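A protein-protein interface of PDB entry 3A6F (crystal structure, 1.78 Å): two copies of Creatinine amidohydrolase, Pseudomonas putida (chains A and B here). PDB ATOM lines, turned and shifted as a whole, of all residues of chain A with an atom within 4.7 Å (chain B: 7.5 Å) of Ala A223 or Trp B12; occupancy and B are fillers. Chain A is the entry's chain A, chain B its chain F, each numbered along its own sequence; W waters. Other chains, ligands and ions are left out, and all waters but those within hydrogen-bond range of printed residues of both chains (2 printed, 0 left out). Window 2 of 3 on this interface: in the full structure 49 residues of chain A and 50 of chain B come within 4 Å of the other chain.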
ATOM      1  N   GLN A  35      -5.926  21.083 -21.995  1.00  0.00           N
ATOM      2  CA  GLN A  35      -4.944  21.133 -23.071  1.00  0.00           C
ATOM      3  C   GLN A  35      -3.576  20.769 -22.515  1.00  0.00           C
ATOM      4  O   GLN A  35      -3.283  21.052 -21.357  1.00  0.00           O
ATOM      5  CB  GLN A  35      -4.897  22.533 -23.712  1.00  0.00           C
ATOM      6  CG  GLN A  35      -4.409  23.679 -22.816  1.00  0.00           C
ATOM      7  CD  GLN A  35      -2.901  23.685 -22.595  1.00  0.00           C
ATOM      8  OE1 GLN A  35      -2.125  23.314 -23.481  1.00  0.00           O
ATOM      9  NE2 GLN A  35      -2.478  24.133 -21.411  1.00  0.00           N
ATOM     10  N   HIS A  36      -2.759  20.125 -23.341  1.00  0.00           N
ATOM     11  CA  HIS A  36      -1.407  19.726 -22.954  1.00  0.00           C
ATOM     12  C   HIS A  36      -0.403  19.954 -24.081  1.00  0.00           C
ATOM     13  O   HIS A  36       0.370  19.055 -24.429  1.00  0.00           O
ATOM     14  CB  HIS A  36      -1.371  18.255 -22.533  1.00  0.00           C
ATOM     15  CG  HIS A  36      -1.712  18.037 -21.095  1.00  0.00           C
ATOM     16  ND1 HIS A  36      -2.981  18.228 -20.593  1.00  0.00           N
ATOM     17  CD2 HIS A  36      -0.934  17.710 -20.038  1.00  0.00           C
ATOM     18  CE1 HIS A  36      -2.968  18.033 -19.285  1.00  0.00           C
ATOM     19  NE2 HIS A  36      -1.737  17.719 -18.926  1.00  0.00           N
ATOM     20  N   GLY A  37      -0.425  21.156 -24.650  1.00  0.00           N
ATOM     21  CA  GLY A  37       0.497  21.497 -25.720  1.00  0.00           C
ATOM     22  C   GLY A  37       0.126  20.960 -27.089  1.00  0.00           C
ATOM     23  O   GLY A  37      -0.949  20.391 -27.279  1.00  0.00           O
ATOM     24  N   HIS A  38       1.026  21.149 -28.051  1.00  0.00           N
ATOM     25  CA  HIS A  38       0.802  20.682 -29.416  1.00  0.00           C
ATOM     26  C   HIS A  38       1.184  19.215 -29.578  1.00  0.00           C
ATOM     27  O   HIS A  38       0.856  18.601 -30.591  1.00  0.00           O
ATOM     28  CB  HIS A  38       1.648  21.489 -30.413  1.00  0.00           C
ATOM     29  CG  HIS A  38       1.387  22.962 -30.398  1.00  0.00           C
ATOM     30  ND1 HIS A  38       2.060  23.840 -31.221  1.00  0.00           N
ATOM     31  CD2 HIS A  38       0.528  23.714 -29.670  1.00  0.00           C
ATOM     32  CE1 HIS A  38       1.626  25.068 -31.001  1.00  0.00           C
ATOM     33  NE2 HIS A  38       0.697  25.019 -30.065  1.00  0.00           N
ATOM     34  N   MET A  42      -5.534  15.589 -24.609  1.00  0.00           N
ATOM     35  CA  MET A  42      -6.083  16.315 -23.471  1.00  0.00           C
ATOM     36  C   MET A  42      -6.576  15.534 -22.253  1.00  0.00           C
ATOM     37  O   MET A  42      -6.935  16.144 -21.251  1.00  0.00           O
ATOM     38  CB  MET A  42      -7.199  17.245 -23.961  1.00  0.00           C
ATOM     39  CG  MET A  42      -6.705  18.297 -24.959  1.00  0.00           C
ATOM     40  SD  MET A  42      -7.989  19.439 -25.440  1.00  0.00           S
ATOM     41  CE  MET A  42      -8.951  18.411 -26.594  1.00  0.00           C
ATOM     42  N   PHE A  84      -8.017  28.424 -22.890  1.00  0.00           N
ATOM     43  CA  PHE A  84      -7.697  27.559 -24.026  1.00  0.00           C
ATOM     44  C   PHE A  84      -8.915  26.743 -24.443  1.00  0.00           C
ATOM     45  O   PHE A  84      -9.796  26.461 -23.628  1.00  0.00           O
ATOM     46  CB  PHE A  84      -6.582  26.558 -23.684  1.00  0.00           C
ATOM     47  CG  PHE A  84      -5.194  27.131 -23.725  1.00  0.00           C
ATOM     48  CD1 PHE A  84      -4.713  27.912 -22.677  1.00  0.00           C
ATOM     49  CD2 PHE A  84      -4.355  26.869 -24.807  1.00  0.00           C
ATOM     50  CE1 PHE A  84      -3.410  28.422 -22.708  1.00  0.00           C
ATOM     51  CE2 PHE A  84      -3.055  27.373 -24.847  1.00  0.00           C
ATOM     52  CZ  PHE A  84      -2.581  28.150 -23.798  1.00  0.00           C
ATOM     53  N   PRO A  85      -8.980  26.362 -25.728  1.00  0.00           N
ATOM     54  CA  PRO A  85     -10.098  25.559 -26.236  1.00  0.00           C
ATOM     55  C   PRO A  85      -9.810  24.145 -25.737  1.00  0.00           C
ATOM     56  O   PRO A  85      -8.678  23.854 -25.345  1.00  0.00           O
ATOM     57  CB  PRO A  85      -9.934  25.640 -27.758  1.00  0.00           C
ATOM     58  CG  PRO A  85      -9.060  26.846 -27.980  1.00  0.00           C
ATOM     59  CD  PRO A  85      -8.102  26.791 -26.830  1.00  0.00           C
ATOM     60  N   THR A 221       0.913  33.281 -20.828  1.00  0.00           N
ATOM     61  CA  THR A 221       1.070  31.837 -20.965  1.00  0.00           C
ATOM     62  C   THR A 221       1.744  31.528 -22.300  1.00  0.00           C
ATOM     63  O   THR A 221       1.381  32.104 -23.327  1.00  0.00           O
ATOM     64  CB  THR A 221      -0.292  31.104 -20.965  1.00  0.00           C
ATOM     65  OG1 THR A 221      -0.965  31.309 -19.716  1.00  0.00           O
ATOM     66  CG2 THR A 221      -0.082  29.613 -21.189  1.00  0.00           C
ATOM     67  N   PRO A 222       2.743  30.627 -22.303  1.00  0.00           N
ATOM     68  CA  PRO A 222       3.412  30.288 -23.562  1.00  0.00           C
ATOM     69  C   PRO A 222       2.350  29.862 -24.580  1.00  0.00           C
ATOM     70  O   PRO A 222       1.395  29.167 -24.231  1.00  0.00           O
ATOM     71  CB  PRO A 222       4.334  29.142 -23.159  1.00  0.00           C
ATOM     72  CG  PRO A 222       4.706  29.505 -21.758  1.00  0.00           C
ATOM     73  CD  PRO A 222       3.380  29.938 -21.169  1.00  0.00           C
ATOM     74  N   ALA A 223       2.525  30.281 -25.829  1.00  0.00           N
ATOM     75  CA  ALA A 223       1.576  29.978 -26.898  1.00  0.00           C
ATOM     76  C   ALA A 223       1.100  28.524 -27.027  1.00  0.00           C
ATOM     77  O   ALA A 223      -0.086  28.275 -27.242  1.00  0.00           O
ATOM     78  CB  ALA A 223       2.149  30.450 -28.237  1.00  0.00           C
ATOM     79  N   PRO A 224       2.013  27.547 -26.904  1.00  0.00           N
ATOM     80  CA  PRO A 224       1.619  26.138 -27.024  1.00  0.00           C
ATOM     81  C   PRO A 224       0.766  25.607 -25.872  1.00  0.00           C
ATOM     82  O   PRO A 224       0.115  24.571 -26.005  1.00  0.00           O
ATOM     83  CB  PRO A 224       2.962  25.404 -27.113  1.00  0.00           C
ATOM     84  CG  PRO A 224       3.911  26.453 -27.609  1.00  0.00           C
ATOM     85  CD  PRO A 224       3.478  27.665 -26.834  1.00  0.00           C
ATOM     86  N   GLY A 225       0.772  26.309 -24.745  1.00  0.00           N
ATOM     87  CA  GLY A 225      -0.001  25.853 -23.606  1.00  0.00           C
ATOM     88  C   GLY A 225       0.885  25.194 -22.563  1.00  0.00           C
ATOM     89  O   GLY A 225       0.508  25.070 -21.397  1.00  0.00           O
ATOM     90  N   VAL B   7     -12.517  13.358 -28.038  1.00  0.00           N
ATOM     91  CA  VAL B   7     -11.926  14.646 -27.689  1.00  0.00           C
ATOM     92  C   VAL B   7     -10.716  14.473 -26.763  1.00  0.00           C
ATOM     93  O   VAL B   7      -9.726  15.195 -26.883  1.00  0.00           O
ATOM     94  CB  VAL B   7     -12.969  15.554 -26.993  1.00  0.00           C
ATOM     95  CG1 VAL B   7     -12.317  16.867 -26.536  1.00  0.00           C
ATOM     96  CG2 VAL B   7     -14.126  15.838 -27.956  1.00  0.00           C
ATOM     97  N   LEU B  10      -7.311  13.903 -28.495  1.00  0.00           N
ATOM     98  CA  LEU B  10      -6.847  14.919 -29.434  1.00  0.00           C
ATOM     99  C   LEU B  10      -6.051  15.989 -28.695  1.00  0.00           C
ATOM    100  O   LEU B  10      -6.163  16.129 -27.476  1.00  0.00           O
ATOM    101  CB  LEU B  10      -8.037  15.605 -30.114  1.00  0.00           C
ATOM    102  CG  LEU B  10      -9.086  14.770 -30.843  1.00  0.00           C
ATOM    103  CD1 LEU B  10     -10.176  15.702 -31.345  1.00  0.00           C
ATOM    104  CD2 LEU B  10      -8.453  14.007 -31.994  1.00  0.00           C
ATOM    105  N   THR B  11      -5.248  16.745 -29.433  1.00  0.00           N
ATOM    106  CA  THR B  11      -4.491  17.842 -28.839  1.00  0.00           C
ATOM    107  C   THR B  11      -5.462  19.019 -28.893  1.00  0.00           C
ATOM    108  O   THR B  11      -6.451  18.960 -29.619  1.00  0.00           O
ATOM    109  CB  THR B  11      -3.251  18.191 -29.669  1.00  0.00           C
ATOM    110  OG1 THR B  11      -3.661  18.658 -30.961  1.00  0.00           O
ATOM    111  CG2 THR B  11      -2.356  16.971 -29.824  1.00  0.00           C
ATOM    112  N   TRP B  12      -5.204  20.089 -28.147  1.00  0.00           N
ATOM    113  CA  TRP B  12      -6.134  21.208 -28.189  1.00  0.00           C
ATOM    114  C   TRP B  12      -6.145  21.885 -29.559  1.00  0.00           C
ATOM    115  O   TRP B  12      -7.148  22.482 -29.948  1.00  0.00           O
ATOM    116  CB  TRP B  12      -5.837  22.228 -27.082  1.00  0.00           C
ATOM    117  CG  TRP B  12      -4.607  23.070 -27.257  1.00  0.00           C
ATOM    118  CD1 TRP B  12      -3.344  22.786 -26.822  1.00  0.00           C
ATOM    119  CD2 TRP B  12      -4.546  24.371 -27.847  1.00  0.00           C
ATOM    120  NE1 TRP B  12      -2.500  23.839 -27.097  1.00  0.00           N
ATOM    121  CE2 TRP B  12      -3.214  24.824 -27.728  1.00  0.00           C
ATOM    122  CE3 TRP B  12      -5.492  25.202 -28.466  1.00  0.00           C
ATOM    123  CZ2 TRP B  12      -2.800  26.075 -28.203  1.00  0.00           C
ATOM    124  CZ3 TRP B  12      -5.082  26.447 -28.938  1.00  0.00           C
ATOM    125  CH2 TRP B  12      -3.746  26.870 -28.802  1.00  0.00           C
ATOM    126  N   LYS B  13      -5.040  21.777 -30.291  1.00  0.00           N
ATOM    127  CA  LYS B  13      -4.957  22.369 -31.631  1.00  0.00           C
ATOM    128  C   LYS B  13      -5.883  21.600 -32.568  1.00  0.00           C
ATOM    129  O   LYS B  13      -6.615  22.197 -33.362  1.00  0.00           O
ATOM    130  CB  LYS B  13      -3.525  22.314 -32.170  1.00  0.00           C
ATOM    131  CG  LYS B  13      -2.518  23.121 -31.368  1.00  0.00           C
ATOM    132  CD  LYS B  13      -2.932  24.575 -31.250  1.00  0.00           C
ATOM    133  CE  LYS B  13      -2.962  25.268 -32.604  1.00  0.00           C
ATOM    134  NZ  LYS B  13      -3.406  26.684 -32.474  1.00  0.00           N
ATOM    135  N   GLU B  14      -5.855  20.276 -32.472  1.00  0.00           N
ATOM    136  CA  GLU B  14      -6.720  19.456 -33.309  1.00  0.00           C
ATOM    137  C   GLU B  14      -8.179  19.778 -32.999  1.00  0.00           C
ATOM    138  O   GLU B  14      -8.987  19.962 -33.905  1.00  0.00           O
ATOM    139  CB  GLU B  14      -6.436  17.972 -33.073  1.00  0.00           C
ATOM    140  CG  GLU B  14      -5.002  17.581 -33.411  1.00  0.00           C
ATOM    141  CD  GLU B  14      -4.717  16.106 -33.209  1.00  0.00           C
ATOM    142  OE1 GLU B  14      -5.008  15.574 -32.114  1.00  0.00           O
ATOM    143  OE2 GLU B  14      -4.188  15.481 -34.152  1.00  0.00           O
ATOM    144  N   TYR B  15      -8.512  19.855 -31.712  1.00  0.00           N
ATOM    145  CA  TYR B  15      -9.871  20.176 -31.294  1.00  0.00           C
ATOM    146  C   TYR B  15     -10.296  21.549 -31.830  1.00  0.00           C
ATOM    147  O   TYR B  15     -11.383  21.703 -32.391  1.00  0.00           O
ATOM    148  CB  TYR B  15      -9.956  20.173 -29.762  1.00  0.00           C
ATOM    149  CG  TYR B  15     -11.310  20.573 -29.222  1.00  0.00           C
ATOM    150  CD1 TYR B  15     -12.409  19.719 -29.335  1.00  0.00           C
ATOM    151  CD2 TYR B  15     -11.496  21.814 -28.609  1.00  0.00           C
ATOM    152  CE1 TYR B  15     -13.666  20.092 -28.848  1.00  0.00           C
ATOM    153  CE2 TYR B  15     -12.747  22.198 -28.120  1.00  0.00           C
ATOM    154  CZ  TYR B  15     -13.826  21.331 -28.242  1.00  0.00           C
ATOM    155  OH  TYR B  15     -15.060  21.702 -27.759  1.00  0.00           O
ATOM    156  N   GLU B  16      -9.433  22.545 -31.642  1.00  0.00           N
ATOM    157  CA  GLU B  16      -9.714  23.902 -32.093  1.00  0.00           C
ATOM    158  C   GLU B  16     -10.002  23.952 -33.591  1.00  0.00           C
ATOM    159  O   GLU B  16     -10.937  24.625 -34.031  1.00  0.00           O
ATOM    160  CB  GLU B  16      -8.533  24.820 -31.765  1.00  0.00           C
ATOM    161  CG  GLU B  16      -8.746  26.274 -32.168  1.00  0.00           C
ATOM    162  CD  GLU B  16      -7.557  27.151 -31.834  1.00  0.00           C
ATOM    163  OE1 GLU B  16      -6.458  26.896 -32.371  1.00  0.00           O
ATOM    164  OE2 GLU B  16      -7.717  28.092 -31.029  1.00  0.00           O
ATOM    165  N   ALA B  17      -9.191  23.244 -34.371  1.00  0.00           N
ATOM    166  CA  ALA B  17      -9.366  23.210 -35.819  1.00  0.00           C
ATOM    167  C   ALA B  17     -10.746  22.670 -36.173  1.00  0.00           C
ATOM    168  O   ALA B  17     -11.432  23.217 -37.036  1.00  0.00           O
ATOM    169  CB  ALA B  17      -8.284  22.344 -36.456  1.00  0.00           C
ATOM    170  N   ARG B  18     -11.155  21.600 -35.496  1.00  0.00           N
ATOM    171  CA  ARG B  18     -12.457  20.999 -35.757  1.00  0.00           C
ATOM    172  C   ARG B  18     -13.615  21.923 -35.396  1.00  0.00           C
ATOM    173  O   ARG B  18     -14.599  22.010 -36.131  1.00  0.00           O
ATOM    174  CB  ARG B  18     -12.590  19.672 -35.002  1.00  0.00           C
ATOM    175  CG  ARG B  18     -11.735  18.555 -35.569  1.00  0.00           C
ATOM    176  CD  ARG B  18     -12.121  18.240 -37.012  1.00  0.00           C
ATOM    177  NE  ARG B  18     -13.431  17.600 -37.120  1.00  0.00           N
ATOM    178  CZ  ARG B  18     -13.685  16.342 -36.761  1.00  0.00           C
ATOM    179  NH1 ARG B  18     -12.720  15.580 -36.265  1.00  0.00           N
ATOM    180  NH2 ARG B  18     -14.905  15.842 -36.899  1.00  0.00           N
HETATM  181  O   HOH W   1      -3.082  19.298 -26.070  1.00  0.00           O
HETATM  182  O   HOH W   2      -1.221  19.379 -32.251  1.00  0.00           O
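The backbone carbonyl oxygen (O) of Leu B10 is in hydrogen-bond range of the backbone NH (N) of Met A42 (3.0 Å). The backbone carbonyl oxygen of Pro A224 sits at hydrogen-bond distance from the indole nitrogen of Trp B12.
NZ of Lys B13 is in salt-bridge range of OE1 of Glu B16 (3.1 Å). OG1 of Thr B11 lies close to N of Lys B13, at 3.5 Å. The side-chain amide nitrogen of Gln A35 is in hydrogen-bond range of the backbone carbonyl oxygen of Gly A225, at 3.1 Å. The side-chain carboxylate (OE1) of Glu B14 sits at hydrogen-bond distance from the backbone NH (N) of Thr B11, at 2.9 Å. The backbone NH (N) of Gly A37 is in hydrogen-bond range of the side-chain amide oxygen (OE1) of Gln A35 (3.0 Å).
Among the printed residues, merely in contact across the chains: Met A42 with Val B7 (3.3 Å), Gly A37 with Trp B12 (3.4 Å), Pro A85 with Trp B12 (3.5 Å), Gln A35 with Trp B12 (3.5 Å), His A38 with Lys B13 (3.5 Å), Pro A85 with Glu B16 (3.6 Å), Phe A84 with Trp B12 (3.6 Å), Ala A223 with Trp B12 (3.6 Å), His A38 with Thr B11 (3.7 Å), Met A42 with Trp B12 (3.8 Å), Met A42 with Tyr B15 (3.8 Å), Met A42 with Thr B11 (3.96 Å), His A38 with Trp B12 (3.98 Å) and Gly A37 with Thr B11 (3.98 Å).
Of the printed residues of chain B, Gly A37 touches Thr B11 and Trp B12. Printed residues of chain B within 4 Å of Phe A84: Trp B12 (3.6 Å). Thr A221 touches none of the printed residues of chain B. Pro A222 touches none of the printed residues of chain B. Ala A223 touches just one residue of chain B: Trp B12. Of the printed residues of chain A, Val B7 touches Met A42 (3.3 Å). Of the printed residues of chain A, Trp B12 touches Gln A35 (3.5 Å), Gly A37 (3.4 Å), His A38 (3.98 Å), Met A42 (3.8 Å), Phe A84 (3.6 Å), Pro A85 (3.5 Å), Ala A223 (3.6 Å) and Pro A224 (2.9 Å). Of the printed residues of chain A, Lys B13 touches His A38 (3.5 Å). The nearest residue of chain A that does not touch Trp B12 is His A36 (4.4 Å).
Of the 10 printed residues of chain B, 7 touch a printed residue of chain A. Hydrophobic or aromatic side chains of chain B that line the printed part of chain A: Val B7, Trp B12 and Tyr B15. Printed residues of chain A that touch a printed residue of chain B: Gln A35, Gly A37, His A38, Met A42, Phe A84, Pro A85, Ala A223 and Pro A224. Among the printed residues, 16 pairs touch across the chains.
No position is printed for both chains. Of the 16 pairs that touch across the chains among the printed residues, none has its exchanged pair printed and touching as well.
Water W1 lies within hydrogen-bond range of O of Gly A37 (2.7 Å), N of His A36 (2.9 Å) and N of Trp B12 (3.1 Å). Water W2 bridges the backbone carbonyl oxygen (O) of His A38 (2.8 Å) and the side-chain hydroxyl (OG1) of Thr B11 (2.9 Å).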
